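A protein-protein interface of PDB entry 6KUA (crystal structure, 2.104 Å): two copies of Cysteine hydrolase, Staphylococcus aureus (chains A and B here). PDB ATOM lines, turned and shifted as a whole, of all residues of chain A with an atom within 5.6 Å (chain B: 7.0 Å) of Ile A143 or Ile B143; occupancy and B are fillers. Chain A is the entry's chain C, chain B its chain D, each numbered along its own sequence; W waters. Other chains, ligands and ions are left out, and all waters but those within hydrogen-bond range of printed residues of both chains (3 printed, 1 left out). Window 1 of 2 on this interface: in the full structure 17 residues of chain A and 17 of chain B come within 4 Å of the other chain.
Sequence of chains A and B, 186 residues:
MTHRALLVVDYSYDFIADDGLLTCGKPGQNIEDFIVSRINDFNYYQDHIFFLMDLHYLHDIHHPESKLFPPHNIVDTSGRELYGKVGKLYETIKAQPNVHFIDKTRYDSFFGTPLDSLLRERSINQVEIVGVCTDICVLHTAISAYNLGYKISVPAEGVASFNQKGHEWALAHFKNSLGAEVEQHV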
ATOM      1  N   VAL A 138     -13.006  29.490 -20.064  1.00  0.00           N
ATOM      2  CA  VAL A 138     -12.299  28.935 -21.216  1.00  0.00           C
ATOM      3  C   VAL A 138     -13.255  28.112 -22.068  1.00  0.00           C
ATOM      4  O   VAL A 138     -13.252  28.195 -23.305  1.00  0.00           O
ATOM      5  CB  VAL A 138     -11.096  28.097 -20.758  1.00  0.00           C
ATOM      6  CG1 VAL A 138     -10.565  27.252 -21.935  1.00  0.00           C
ATOM      7  CG2 VAL A 138      -9.988  29.001 -20.173  1.00  0.00           C
ATOM      8  N   LEU A 139     -14.072  27.295 -21.403  1.00  0.00           N
ATOM      9  CA  LEU A 139     -15.073  26.466 -22.064  1.00  0.00           C
ATOM     10  C   LEU A 139     -16.025  27.305 -22.909  1.00  0.00           C
ATOM     11  O   LEU A 139     -16.221  27.023 -24.093  1.00  0.00           O
ATOM     12  CB  LEU A 139     -15.859  25.677 -21.014  1.00  0.00           C
ATOM     13  CG  LEU A 139     -17.103  24.969 -21.560  1.00  0.00           C
ATOM     14  CD1 LEU A 139     -16.725  23.884 -22.579  1.00  0.00           C
ATOM     15  CD2 LEU A 139     -17.922  24.390 -20.408  1.00  0.00           C
ATOM     16  N   HIS A 140     -16.651  28.318 -22.300  1.00  0.00           N
ATOM     17  CA  HIS A 140     -17.616  29.142 -23.029  1.00  0.00           C
ATOM     18  C   HIS A 140     -16.933  29.900 -24.160  1.00  0.00           C
ATOM     19  O   HIS A 140     -17.457  29.976 -25.281  1.00  0.00           O
ATOM     20  CB  HIS A 140     -18.311  30.135 -22.091  1.00  0.00           C
ATOM     21  CG  HIS A 140     -19.160  29.510 -21.025  1.00  0.00           C
ATOM     22  ND1 HIS A 140     -20.173  30.206 -20.400  1.00  0.00           N
ATOM     23  CD2 HIS A 140     -19.111  28.299 -20.418  1.00  0.00           C
ATOM     24  CE1 HIS A 140     -20.735  29.440 -19.478  1.00  0.00           C
ATOM     25  NE2 HIS A 140     -20.105  28.281 -19.464  1.00  0.00           N
ATOM     26  N   THR A 141     -15.755  30.471 -23.882  1.00  0.00           N
ATOM     27  CA  THR A 141     -14.979  31.100 -24.948  1.00  0.00           C
ATOM     28  C   THR A 141     -14.711  30.121 -26.083  1.00  0.00           C
ATOM     29  O   THR A 141     -14.882  30.464 -27.255  1.00  0.00           O
ATOM     30  CB  THR A 141     -13.672  31.644 -24.387  1.00  0.00           C
ATOM     31  OG1 THR A 141     -13.977  32.662 -23.434  1.00  0.00           O
ATOM     32  CG2 THR A 141     -12.762  32.209 -25.522  1.00  0.00           C
ATOM     33  N   ALA A 142     -14.312  28.887 -25.753  1.00  0.00           N
ATOM     34  CA  ALA A 142     -13.978  27.897 -26.776  1.00  0.00           C
ATOM     35  C   ALA A 142     -15.201  27.461 -27.576  1.00  0.00           C
ATOM     36  O   ALA A 142     -15.104  27.240 -28.786  1.00  0.00           O
ATOM     37  CB  ALA A 142     -13.321  26.674 -26.131  1.00  0.00           C
ATOM     38  N   ILE A 143     -16.349  27.289 -26.915  1.00  0.00           N
ATOM     39  CA  ILE A 143     -17.566  26.912 -27.633  1.00  0.00           C
ATOM     40  C   ILE A 143     -17.923  27.973 -28.677  1.00  0.00           C
ATOM     41  O   ILE A 143     -18.264  27.655 -29.824  1.00  0.00           O
ATOM     42  CB  ILE A 143     -18.709  26.684 -26.625  1.00  0.00           C
ATOM     43  CG1 ILE A 143     -18.491  25.378 -25.851  1.00  0.00           C
ATOM     44  CG2 ILE A 143     -20.087  26.702 -27.326  1.00  0.00           C
ATOM     45  CD1 ILE A 143     -19.435  25.214 -24.643  1.00  0.00           C
ATOM     46  N   SER A 144     -17.827  29.251 -28.302  1.00  0.00           N
ATOM     47  CA  SER A 144     -18.144  30.331 -29.239  1.00  0.00           C
ATOM     48  C   SER A 144     -17.153  30.380 -30.398  1.00  0.00           C
ATOM     49  O   SER A 144     -17.553  30.583 -31.560  1.00  0.00           O
ATOM     50  CB  SER A 144     -18.170  31.662 -28.498  1.00  0.00           C
ATOM     51  OG  SER A 144     -19.368  31.808 -27.766  1.00  0.00           O
ATOM     52  N   ALA A 145     -15.854  30.206 -30.102  1.00  0.00           N
ATOM     53  CA  ALA A 145     -14.864  30.151 -31.179  1.00  0.00           C
ATOM     54  C   ALA A 145     -15.179  29.010 -32.141  1.00  0.00           C
ATOM     55  O   ALA A 145     -15.046  29.159 -33.364  1.00  0.00           O
ATOM     56  CB  ALA A 145     -13.450  29.989 -30.612  1.00  0.00           C
ATOM     57  N   TYR A 146     -15.613  27.871 -31.599  1.00  0.00           N
ATOM     58  CA  TYR A 146     -15.973  26.717 -32.424  1.00  0.00           C
ATOM     59  C   TYR A 146     -17.162  27.035 -33.321  1.00  0.00           C
ATOM     60  O   TYR A 146     -17.129  26.788 -34.533  1.00  0.00           O
ATOM     61  CB  TYR A 146     -16.274  25.516 -31.520  1.00  0.00           C
ATOM     62  CG  TYR A 146     -17.058  24.411 -32.192  1.00  0.00           C
ATOM     63  CD1 TYR A 146     -16.413  23.436 -32.933  1.00  0.00           C
ATOM     64  CD2 TYR A 146     -18.458  24.353 -32.096  1.00  0.00           C
ATOM     65  CE1 TYR A 146     -17.119  22.419 -33.555  1.00  0.00           C
ATOM     66  CE2 TYR A 146     -19.186  23.343 -32.728  1.00  0.00           C
ATOM     67  CZ  TYR A 146     -18.499  22.381 -33.459  1.00  0.00           C
ATOM     68  OH  TYR A 146     -19.173  21.376 -34.095  1.00  0.00           O
ATOM     69  N   ASN A 147     -18.228  27.583 -32.731  1.00  0.00           N
ATOM     70  CA  ASN A 147     -19.421  27.935 -33.497  1.00  0.00           C
ATOM     71  C   ASN A 147     -19.101  28.938 -34.592  1.00  0.00           C
ATOM     72  O   ASN A 147     -19.662  28.863 -35.688  1.00  0.00           O
ATOM     73  CB  ASN A 147     -20.491  28.514 -32.572  1.00  0.00           C
ATOM     74  CG  ASN A 147     -21.228  27.443 -31.798  1.00  0.00           C
ATOM     75  OD1 ASN A 147     -21.233  26.277 -32.192  1.00  0.00           O
ATOM     76  ND2 ASN A 147     -21.869  27.838 -30.693  1.00  0.00           N
ATOM     77  N   LEU A 148     -18.205  29.890 -34.308  1.00  0.00           N
ATOM     78  CA  LEU A 148     -17.822  30.919 -35.267  1.00  0.00           C
ATOM     79  C   LEU A 148     -16.814  30.424 -36.295  1.00  0.00           C
ATOM     80  O   LEU A 148     -16.349  31.222 -37.113  1.00  0.00           O
ATOM     81  CB  LEU A 148     -17.260  32.141 -34.533  1.00  0.00           C
ATOM     82  CG  LEU A 148     -18.284  32.882 -33.667  1.00  0.00           C
ATOM     83  CD1 LEU A 148     -17.589  33.927 -32.790  1.00  0.00           C
ATOM     84  CD2 LEU A 148     -19.368  33.518 -34.536  1.00  0.00           C
ATOM     85  N   HIS A 173     -13.736  17.436 -23.827  1.00  0.00           N
ATOM     86  CA  HIS A 173     -14.787  18.067 -24.629  1.00  0.00           C
ATOM     87  C   HIS A 173     -14.192  18.830 -25.814  1.00  0.00           C
ATOM     88  O   HIS A 173     -14.672  18.696 -26.948  1.00  0.00           O
ATOM     89  CB  HIS A 173     -15.625  19.001 -23.745  1.00  0.00           C
ATOM     90  CG  HIS A 173     -16.822  19.581 -24.434  1.00  0.00           C
ATOM     91  ND1 HIS A 173     -17.934  18.829 -24.742  1.00  0.00           N
ATOM     92  CD2 HIS A 173     -17.088  20.838 -24.865  1.00  0.00           C
ATOM     93  CE1 HIS A 173     -18.831  19.594 -25.341  1.00  0.00           C
ATOM     94  NE2 HIS A 173     -18.343  20.818 -25.423  1.00  0.00           N
ATOM     95  N   LEU A 178     -15.337  19.699 -29.958  1.00  0.00           N
ATOM     96  CA  LEU A 178     -14.975  20.935 -30.636  1.00  0.00           C
ATOM     97  C   LEU A 178     -13.830  20.775 -31.629  1.00  0.00           C
ATOM     98  O   LEU A 178     -13.407  21.774 -32.212  1.00  0.00           O
ATOM     99  CB  LEU A 178     -14.624  22.016 -29.605  1.00  0.00           C
ATOM    100  CG  LEU A 178     -15.614  22.122 -28.450  1.00  0.00           C
ATOM    101  CD1 LEU A 178     -15.263  23.307 -27.530  1.00  0.00           C
ATOM    102  CD2 LEU A 178     -17.061  22.215 -28.984  1.00  0.00           C
ATOM    103  N   TYR B 107     -24.359  22.256 -32.293  1.00  0.00           N
ATOM    104  CA  TYR B 107     -24.912  21.702 -31.062  1.00  0.00           C
ATOM    105  C   TYR B 107     -25.855  22.693 -30.388  1.00  0.00           C
ATOM    106  O   TYR B 107     -26.893  22.304 -29.840  1.00  0.00           O
ATOM    107  CB  TYR B 107     -23.798  21.322 -30.091  1.00  0.00           C
ATOM    108  CG  TYR B 107     -22.681  20.454 -30.657  1.00  0.00           C
ATOM    109  CD1 TYR B 107     -22.933  19.192 -31.176  1.00  0.00           C
ATOM    110  CD2 TYR B 107     -21.369  20.904 -30.637  1.00  0.00           C
ATOM    111  CE1 TYR B 107     -21.892  18.397 -31.667  1.00  0.00           C
ATOM    112  CE2 TYR B 107     -20.321  20.125 -31.117  1.00  0.00           C
ATOM    113  CZ  TYR B 107     -20.588  18.876 -31.632  1.00  0.00           C
ATOM    114  OH  TYR B 107     -19.535  18.114 -32.108  1.00  0.00           O
ATOM    115  N   ASP B 108     -25.493  23.970 -30.417  1.00  0.00           N
ATOM    116  CA  ASP B 108     -26.219  25.044 -29.752  1.00  0.00           C
ATOM    117  C   ASP B 108     -27.519  25.332 -30.501  1.00  0.00           C
ATOM    118  O   ASP B 108     -27.488  25.723 -31.677  1.00  0.00           O
ATOM    119  CB  ASP B 108     -25.312  26.274 -29.714  1.00  0.00           C
ATOM    120  CG  ASP B 108     -25.957  27.506 -29.086  1.00  0.00           C
ATOM    121  OD1 ASP B 108     -27.098  27.444 -28.549  1.00  0.00           O
ATOM    122  OD2 ASP B 108     -25.286  28.562 -29.125  1.00  0.00           O
ATOM    123  N   PHE B 110     -29.422  27.804 -30.299  1.00  0.00           N
ATOM    124  CA  PHE B 110     -29.544  29.218 -30.651  1.00  0.00           C
ATOM    125  C   PHE B 110     -28.665  29.633 -31.828  1.00  0.00           C
ATOM    126  O   PHE B 110     -28.880  30.716 -32.394  1.00  0.00           O
ATOM    127  CB  PHE B 110     -29.184  30.101 -29.445  1.00  0.00           C
ATOM    128  CG  PHE B 110     -30.204  30.063 -28.334  1.00  0.00           C
ATOM    129  CD1 PHE B 110     -30.128  29.097 -27.329  1.00  0.00           C
ATOM    130  CD2 PHE B 110     -31.255  30.990 -28.302  1.00  0.00           C
ATOM    131  CE1 PHE B 110     -31.075  29.051 -26.302  1.00  0.00           C
ATOM    132  CE2 PHE B 110     -32.209  30.958 -27.284  1.00  0.00           C
ATOM    133  CZ  PHE B 110     -32.123  29.984 -26.277  1.00  0.00           C
ATOM    134  N   ILE B 129     -35.087  23.072 -20.363  1.00  0.00           N
ATOM    135  CA  ILE B 129     -34.364  22.336 -21.399  1.00  0.00           C
ATOM    136  C   ILE B 129     -34.354  20.855 -21.053  1.00  0.00           C
ATOM    137  O   ILE B 129     -33.942  20.469 -19.956  1.00  0.00           O
ATOM    138  CB  ILE B 129     -32.931  22.870 -21.570  1.00  0.00           C
ATOM    139  CG1 ILE B 129     -32.924  24.399 -21.723  1.00  0.00           C
ATOM    140  CG2 ILE B 129     -32.228  22.189 -22.762  1.00  0.00           C
ATOM    141  CD1 ILE B 129     -31.460  24.996 -21.786  1.00  0.00           C
ATOM    142  N   ILE B 136     -23.396  18.095 -24.125  1.00  0.00           N
ATOM    143  CA  ILE B 136     -23.095  18.605 -25.463  1.00  0.00           C
ATOM    144  C   ILE B 136     -24.202  19.553 -25.935  1.00  0.00           C
ATOM    145  O   ILE B 136     -24.163  20.755 -25.652  1.00  0.00           O
ATOM    146  CB  ILE B 136     -22.863  17.459 -26.461  1.00  0.00           C
ATOM    147  CG1 ILE B 136     -21.923  16.401 -25.853  1.00  0.00           C
ATOM    148  CG2 ILE B 136     -22.277  18.021 -27.773  1.00  0.00           C
ATOM    149  CD1 ILE B 136     -21.500  15.285 -26.813  1.00  0.00           C
ATOM    150  N   CYS B 137     -25.204  19.030 -26.648  1.00  0.00           N
ATOM    151  CA  CYS B 137     -26.252  19.908 -27.182  1.00  0.00           C
ATOM    152  C   CYS B 137     -27.000  20.636 -26.067  1.00  0.00           C
ATOM    153  O   CYS B 137     -27.222  21.847 -26.158  1.00  0.00           O
ATOM    154  CB  CYS B 137     -27.215  19.110 -28.073  1.00  0.00           C
ATOM    155  SG  CYS B 137     -26.427  18.576 -29.660  1.00  0.00           S
ATOM    156  N   VAL B 138     -27.349  19.936 -24.984  1.00  0.00           N
ATOM    157  CA  VAL B 138     -28.007  20.612 -23.863  1.00  0.00           C
ATOM    158  C   VAL B 138     -27.084  21.666 -23.261  1.00  0.00           C
ATOM    159  O   VAL B 138     -27.511  22.779 -22.925  1.00  0.00           O
ATOM    160  CB  VAL B 138     -28.455  19.582 -22.800  1.00  0.00           C
ATOM    161  CG1 VAL B 138     -29.004  20.276 -21.535  1.00  0.00           C
ATOM    162  CG2 VAL B 138     -29.464  18.600 -23.361  1.00  0.00           C
ATOM    163  N   LEU B 139     -25.805  21.331 -23.099  1.00  0.00           N
ATOM    164  CA  LEU B 139     -24.867  22.280 -22.494  1.00  0.00           C
ATOM    165  C   LEU B 139     -24.696  23.538 -23.348  1.00  0.00           C
ATOM    166  O   LEU B 139     -24.719  24.657 -22.823  1.00  0.00           O
ATOM    167  CB  LEU B 139     -23.512  21.610 -22.267  1.00  0.00           C
ATOM    168  CG  LEU B 139     -22.364  22.573 -21.965  1.00  0.00           C
ATOM    169  CD1 LEU B 139     -22.535  23.166 -20.588  1.00  0.00           C
ATOM    170  CD2 LEU B 139     -21.013  21.844 -22.099  1.00  0.00           C
ATOM    171  N   HIS B 140     -24.489  23.378 -24.659  1.00  0.00           N
ATOM    172  CA  HIS B 140     -24.277  24.552 -25.514  1.00  0.00           C
ATOM    173  C   HIS B 140     -25.531  25.417 -25.590  1.00  0.00           C
ATOM    174  O   HIS B 140     -25.445  26.654 -25.612  1.00  0.00           O
ATOM    175  CB  HIS B 140     -23.861  24.121 -26.919  1.00  0.00           C
ATOM    176  CG  HIS B 140     -22.497  23.506 -26.991  1.00  0.00           C
ATOM    177  ND1 HIS B 140     -21.735  23.524 -28.142  1.00  0.00           N
ATOM    178  CD2 HIS B 140     -21.762  22.845 -26.065  1.00  0.00           C
ATOM    179  CE1 HIS B 140     -20.599  22.885 -27.925  1.00  0.00           C
ATOM    180  NE2 HIS B 140     -20.590  22.465 -26.671  1.00  0.00           N
ATOM    181  N   THR B 141     -26.711  24.776 -25.619  1.00  0.00           N
ATOM    182  CA  THR B 141     -27.972  25.506 -25.644  1.00  0.00           C
ATOM    183  C   THR B 141     -28.190  26.267 -24.341  1.00  0.00           C
ATOM    184  O   THR B 141     -28.622  27.426 -24.359  1.00  0.00           O
ATOM    185  CB  THR B 141     -29.130  24.534 -25.905  1.00  0.00           C
ATOM    186  OG1 THR B 141     -28.934  23.863 -27.160  1.00  0.00           O
ATOM    187  CG2 THR B 141     -30.482  25.276 -25.919  1.00  0.00           C
ATOM    188  N   ALA B 142     -27.891  25.625 -23.203  1.00  0.00           N
ATOM    189  CA  ALA B 142     -28.045  26.267 -21.901  1.00  0.00           C
ATOM    190  C   ALA B 142     -27.132  27.479 -21.746  1.00  0.00           C
ATOM    191  O   ALA B 142     -27.539  28.497 -21.169  1.00  0.00           O
ATOM    192  CB  ALA B 142     -27.765  25.258 -20.786  1.00  0.00           C
ATOM    193  N   ILE B 143     -25.881  27.379 -22.226  1.00  0.00           N
ATOM    194  CA  ILE B 143     -24.960  28.507 -22.121  1.00  0.00           C
ATOM    195  C   ILE B 143     -25.465  29.680 -22.944  1.00  0.00           C
ATOM    196  O   ILE B 143     -25.460  30.829 -22.485  1.00  0.00           O
ATOM    197  CB  ILE B 143     -23.544  28.101 -22.564  1.00  0.00           C
ATOM    198  CG1 ILE B 143     -22.942  27.109 -21.581  1.00  0.00           C
ATOM    199  CG2 ILE B 143     -22.663  29.324 -22.686  1.00  0.00           C
ATOM    200  CD1 ILE B 143     -21.832  26.348 -22.177  1.00  0.00           C
ATOM    201  N   SER B 144     -25.897  29.415 -24.179  1.00  0.00           N
ATOM    202  CA  SER B 144     -26.458  30.493 -24.991  1.00  0.00           C
ATOM    203  C   SER B 144     -27.673  31.119 -24.314  1.00  0.00           C
ATOM    204  O   SER B 144     -27.799  32.350 -24.251  1.00  0.00           O
ATOM    205  CB  SER B 144     -26.831  29.977 -26.372  1.00  0.00           C
ATOM    206  OG  SER B 144     -25.700  30.027 -27.221  1.00  0.00           O
ATOM    207  N   ALA B 145     -28.580  30.280 -23.792  1.00  0.00           N
ATOM    208  CA  ALA B 145     -29.744  30.800 -23.077  1.00  0.00           C
ATOM    209  C   ALA B 145     -29.306  31.668 -21.910  1.00  0.00           C
ATOM    210  O   ALA B 145     -29.858  32.747 -21.679  1.00  0.00           O
ATOM    211  CB  ALA B 145     -30.636  29.649 -22.582  1.00  0.00           C
ATOM    212  N   TYR B 146     -28.313  31.199 -21.153  1.00  0.00           N
ATOM    213  CA  TYR B 146     -27.804  31.974 -20.031  1.00  0.00           C
ATOM    214  C   TYR B 146     -27.284  33.336 -20.504  1.00  0.00           C
ATOM    215  O   TYR B 146     -27.675  34.385 -19.967  1.00  0.00           O
ATOM    216  CB  TYR B 146     -26.705  31.178 -19.316  1.00  0.00           C
ATOM    217  CG  TYR B 146     -25.883  32.024 -18.363  1.00  0.00           C
ATOM    218  CD1 TYR B 146     -26.345  32.298 -17.078  1.00  0.00           C
ATOM    219  CD2 TYR B 146     -24.672  32.577 -18.760  1.00  0.00           C
ATOM    220  CE1 TYR B 146     -25.616  33.072 -16.200  1.00  0.00           C
ATOM    221  CE2 TYR B 146     -23.936  33.359 -17.895  1.00  0.00           C
ATOM    222  CZ  TYR B 146     -24.414  33.606 -16.617  1.00  0.00           C
ATOM    223  OH  TYR B 146     -23.691  34.400 -15.757  1.00  0.00           O
ATOM    224  N   ASN B 147     -26.413  33.337 -21.528  1.00  0.00           N
ATOM    225  CA  ASN B 147     -25.846  34.589 -22.042  1.00  0.00           C
ATOM    226  C   ASN B 147     -26.935  35.563 -22.488  1.00  0.00           C
ATOM    227  O   ASN B 147     -26.842  36.769 -22.231  1.00  0.00           O
ATOM    228  CB  ASN B 147     -24.887  34.302 -23.209  1.00  0.00           C
ATOM    229  CG  ASN B 147     -23.546  33.733 -22.741  1.00  0.00           C
ATOM    230  OD1 ASN B 147     -23.238  33.749 -21.545  1.00  0.00           O
ATOM    231  ND2 ASN B 147     -22.750  33.228 -23.682  1.00  0.00           N
ATOM    232  N   LEU B 148     -27.967  35.059 -23.169  1.00  0.00           N
ATOM    233  CA  LEU B 148     -29.093  35.864 -23.632  1.00  0.00           C
ATOM    234  C   LEU B 148     -30.039  36.298 -22.517  1.00  0.00           C
ATOM    235  O   LEU B 148     -31.055  36.935 -22.822  1.00  0.00           O
ATOM    236  CB  LEU B 148     -29.880  35.085 -24.687  1.00  0.00           C
ATOM    237  CG  LEU B 148     -29.009  34.917 -25.929  1.00  0.00           C
ATOM    238  CD1 LEU B 148     -29.563  33.882 -26.869  1.00  0.00           C
ATOM    239  CD2 LEU B 148     -28.860  36.273 -26.619  1.00  0.00           C
ATOM    240  N   GLY B 149     -29.759  35.961 -21.263  1.00  0.00           N
ATOM    241  CA  GLY B 149     -30.553  36.449 -20.142  1.00  0.00           C
ATOM    242  C   GLY B 149     -31.815  35.669 -19.822  1.00  0.00           C
ATOM    243  O   GLY B 149     -32.689  36.185 -19.116  1.00  0.00           O
ATOM    244  N   ILE B 152     -33.200  29.619 -16.495  1.00  0.00           N
ATOM    245  CA  ILE B 152     -33.026  28.278 -17.028  1.00  0.00           C
ATOM    246  C   ILE B 152     -33.452  27.251 -15.993  1.00  0.00           C
ATOM    247  O   ILE B 152     -33.149  27.376 -14.805  1.00  0.00           O
ATOM    248  CB  ILE B 152     -31.565  28.038 -17.452  1.00  0.00           C
ATOM    249  CG1 ILE B 152     -31.149  29.074 -18.494  1.00  0.00           C
ATOM    250  CG2 ILE B 152     -31.383  26.615 -17.982  1.00  0.00           C
ATOM    251  CD1 ILE B 152     -29.660  29.137 -18.659  1.00  0.00           C
ATOM    252  N   TRP B 169     -21.066  16.432 -14.341  1.00  0.00           N
ATOM    253  CA  TRP B 169     -20.404  17.728 -14.437  1.00  0.00           C
ATOM    254  C   TRP B 169     -21.370  18.775 -14.976  1.00  0.00           C
ATOM    255  O   TRP B 169     -21.469  19.881 -14.432  1.00  0.00           O
ATOM    256  CB  TRP B 169     -19.146  17.658 -15.325  1.00  0.00           C
ATOM    257  CG  TRP B 169     -18.580  19.057 -15.517  1.00  0.00           C
ATOM    258  CD1 TRP B 169     -17.696  19.697 -14.707  1.00  0.00           C
ATOM    259  CD2 TRP B 169     -18.960  20.008 -16.527  1.00  0.00           C
ATOM    260  NE1 TRP B 169     -17.484  20.982 -15.159  1.00  0.00           N
ATOM    261  CE2 TRP B 169     -18.253  21.193 -16.274  1.00  0.00           C
ATOM    262  CE3 TRP B 169     -19.821  19.961 -17.629  1.00  0.00           C
ATOM    263  CZ2 TRP B 169     -18.378  22.320 -17.078  1.00  0.00           C
ATOM    264  CZ3 TRP B 169     -19.958  21.097 -18.419  1.00  0.00           C
ATOM    265  CH2 TRP B 169     -19.242  22.250 -18.140  1.00  0.00           C
ATOM    266  N   HIS B 173     -22.628  22.404 -13.424  1.00  0.00           N
ATOM    267  CA  HIS B 173     -22.363  23.639 -14.164  1.00  0.00           C
ATOM    268  C   HIS B 173     -23.627  24.493 -14.304  1.00  0.00           C
ATOM    269  O   HIS B 173     -23.607  25.702 -14.028  1.00  0.00           O
ATOM    270  CB  HIS B 173     -21.799  23.289 -15.541  1.00  0.00           C
ATOM    271  CG  HIS B 173     -21.334  24.479 -16.331  1.00  0.00           C
ATOM    272  ND1 HIS B 173     -20.136  25.117 -16.082  1.00  0.00           N
ATOM    273  CD2 HIS B 173     -21.896  25.132 -17.378  1.00  0.00           C
ATOM    274  CE1 HIS B 173     -19.985  26.115 -16.935  1.00  0.00           C
ATOM    275  NE2 HIS B 173     -21.038  26.147 -17.731  1.00  0.00           N
ATOM    276  N   PHE B 174     -24.735  23.873 -14.748  1.00  0.00           N
ATOM    277  CA  PHE B 174     -26.013  24.582 -14.880  1.00  0.00           C
ATOM    278  C   PHE B 174     -26.373  25.277 -13.582  1.00  0.00           C
ATOM    279  O   PHE B 174     -26.692  26.467 -13.557  1.00  0.00           O
ATOM    280  CB  PHE B 174     -27.146  23.615 -15.253  1.00  0.00           C
ATOM    281  CG  PHE B 174     -26.927  22.861 -16.536  1.00  0.00           C
ATOM    282  CD1 PHE B 174     -26.061  23.342 -17.512  1.00  0.00           C
ATOM    283  CD2 PHE B 174     -27.586  21.658 -16.760  1.00  0.00           C
ATOM    284  CE1 PHE B 174     -25.847  22.626 -18.685  1.00  0.00           C
ATOM    285  CE2 PHE B 174     -27.393  20.939 -17.933  1.00  0.00           C
ATOM    286  CZ  PHE B 174     -26.521  21.416 -18.894  1.00  0.00           C
ATOM    287  N   LEU B 178     -24.543  28.669 -14.329  1.00  0.00           N
ATOM    288  CA  LEU B 178     -25.606  29.287 -15.110  1.00  0.00           C
ATOM    289  C   LEU B 178     -26.793  29.712 -14.262  1.00  0.00           C
ATOM    290  O   LEU B 178     -27.787  30.181 -14.816  1.00  0.00           O
ATOM    291  CB  LEU B 178     -26.073  28.344 -16.224  1.00  0.00           C
ATOM    292  CG  LEU B 178     -24.967  27.760 -17.106  1.00  0.00           C
ATOM    293  CD1 LEU B 178     -25.578  27.050 -18.294  1.00  0.00           C
ATOM    294  CD2 LEU B 178     -23.935  28.841 -17.570  1.00  0.00           C
HETATM  295  O   HOH W   1     -22.543  24.533 -30.579  1.00  0.00           O
HETATM  296  O   HOH W   2     -20.861  33.062 -20.863  1.00  0.00           O
HETATM  297  O   HOH W   3     -21.820  21.271 -34.203  1.00  0.00           O
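A ring nitrogen (NE2) of His B173 is in hydrogen-bond range of a ring nitrogen (NE2) of His A140 (2.9 Å).
A ring nitrogen (NE2) of His A173 lies within hydrogen-bond range of a ring nitrogen (NE2) of His B140 (3.1 Å).
O of His A173 lies within hydrogen-bond range of N of Leu A178 (3.2 Å).
The backbone carbonyl oxygen (O) of Tyr B107 lies close to the side-chain sulfur (SG) of Cys B137, at 3.8 Å.
The backbone NH (N) of Phe B110 lies within hydrogen-bond range of the side-chain carboxylate (OD1) of Asp B108, 2.9 Å away.
The side-chain hydroxyl of Ser B144 sits at hydrogen-bond distance from the side-chain carboxylate of Asp B108, at 2.4 Å.
O of His B173 is in hydrogen-bond range of N of Leu B178 (3.1 Å).
Among the printed residues, merely in contact across the chains: Leu A139 with Trp B169 (3.4 Å), His A140 with Ile B143 (3.5 Å), His A140 with Leu B178 (3.8 Å), Ile A143 with His B140 (3.6 Å), Ile A143 with Ile B143 (3.6 Å), Tyr A146 with Tyr B107 (3.4 Å), Asn A147 with Asp B108 (3.8 Å) and Leu A178 with His B140 (3.8 Å).
Of the printed residues of chain B, His A140 touches Ile B143, His B173 and Leu B178.
Of the printed residues of chain B, Ile A143 touches His B140 and Ile B143.
Printed residues of chain B within 4 Å of His A173: His B140 (3.1 Å).
Of the printed residues of chain B, Leu A178 touches His B140 (3.8 Å).
Ile B143 touches two residues of chain A.
Ser B144 touches none of the printed residues of chain A.
Ile B152 touches none of the printed residues of chain A.
Of the printed residues of chain A, His B173 touches His A140.
The nearest residue of chain B that does not touch Ile A143 is Leu B139 (4.5 Å).
The nearest residue of chain A that does not touch Ile B143 is Leu A139 (4.7 Å).
Of the 13 printed residues of chain A, 7 touch a printed residue of chain B.
Printed residues of chain A that touch a printed residue of chain B: Leu A139, His A140, Ile A143, Tyr A146, Asn A147, His A173 and Leu A178.
Hydrophobic or aromatic side chains of chain A within 4 Å of the printed part of chain B: Leu A139, His A140, Ile A143, Tyr A146, His A173 and Leu A178.
Of the 23 printed residues of chain B, 7 touch a printed residue of chain A.
His A140 touches Ile B143, and with the chains exchanged Ile A143 touches His B140.
His A140 touches His B173, and with the chains exchanged His A173 touches His B140.
His A140 touches Leu B178, and with the chains exchanged Leu A178 touches His B140.
Ile A143 touches its own counterpart, Ile B143.
Of the 10 pairs that touch across the chains among the printed residues, 7 have their exchanged pair printed and touching as well.
Water W2 lies within hydrogen-bond range of the side-chain amide oxygen (OD1) of Asn B147 (2.6 Å) and a ring nitrogen (ND1) of His A140 (3.0 Å).
Water W3 lies within hydrogen-bond range of the side-chain hydroxyl of Tyr A146 (2.7 Å) and the backbone NH of Tyr B107 (3.3 Å).
Water W1 lies within hydrogen-bond range of OD1 of Asn A147, ND1 of His B140, N of Asp B108 and N of Tyr B107.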
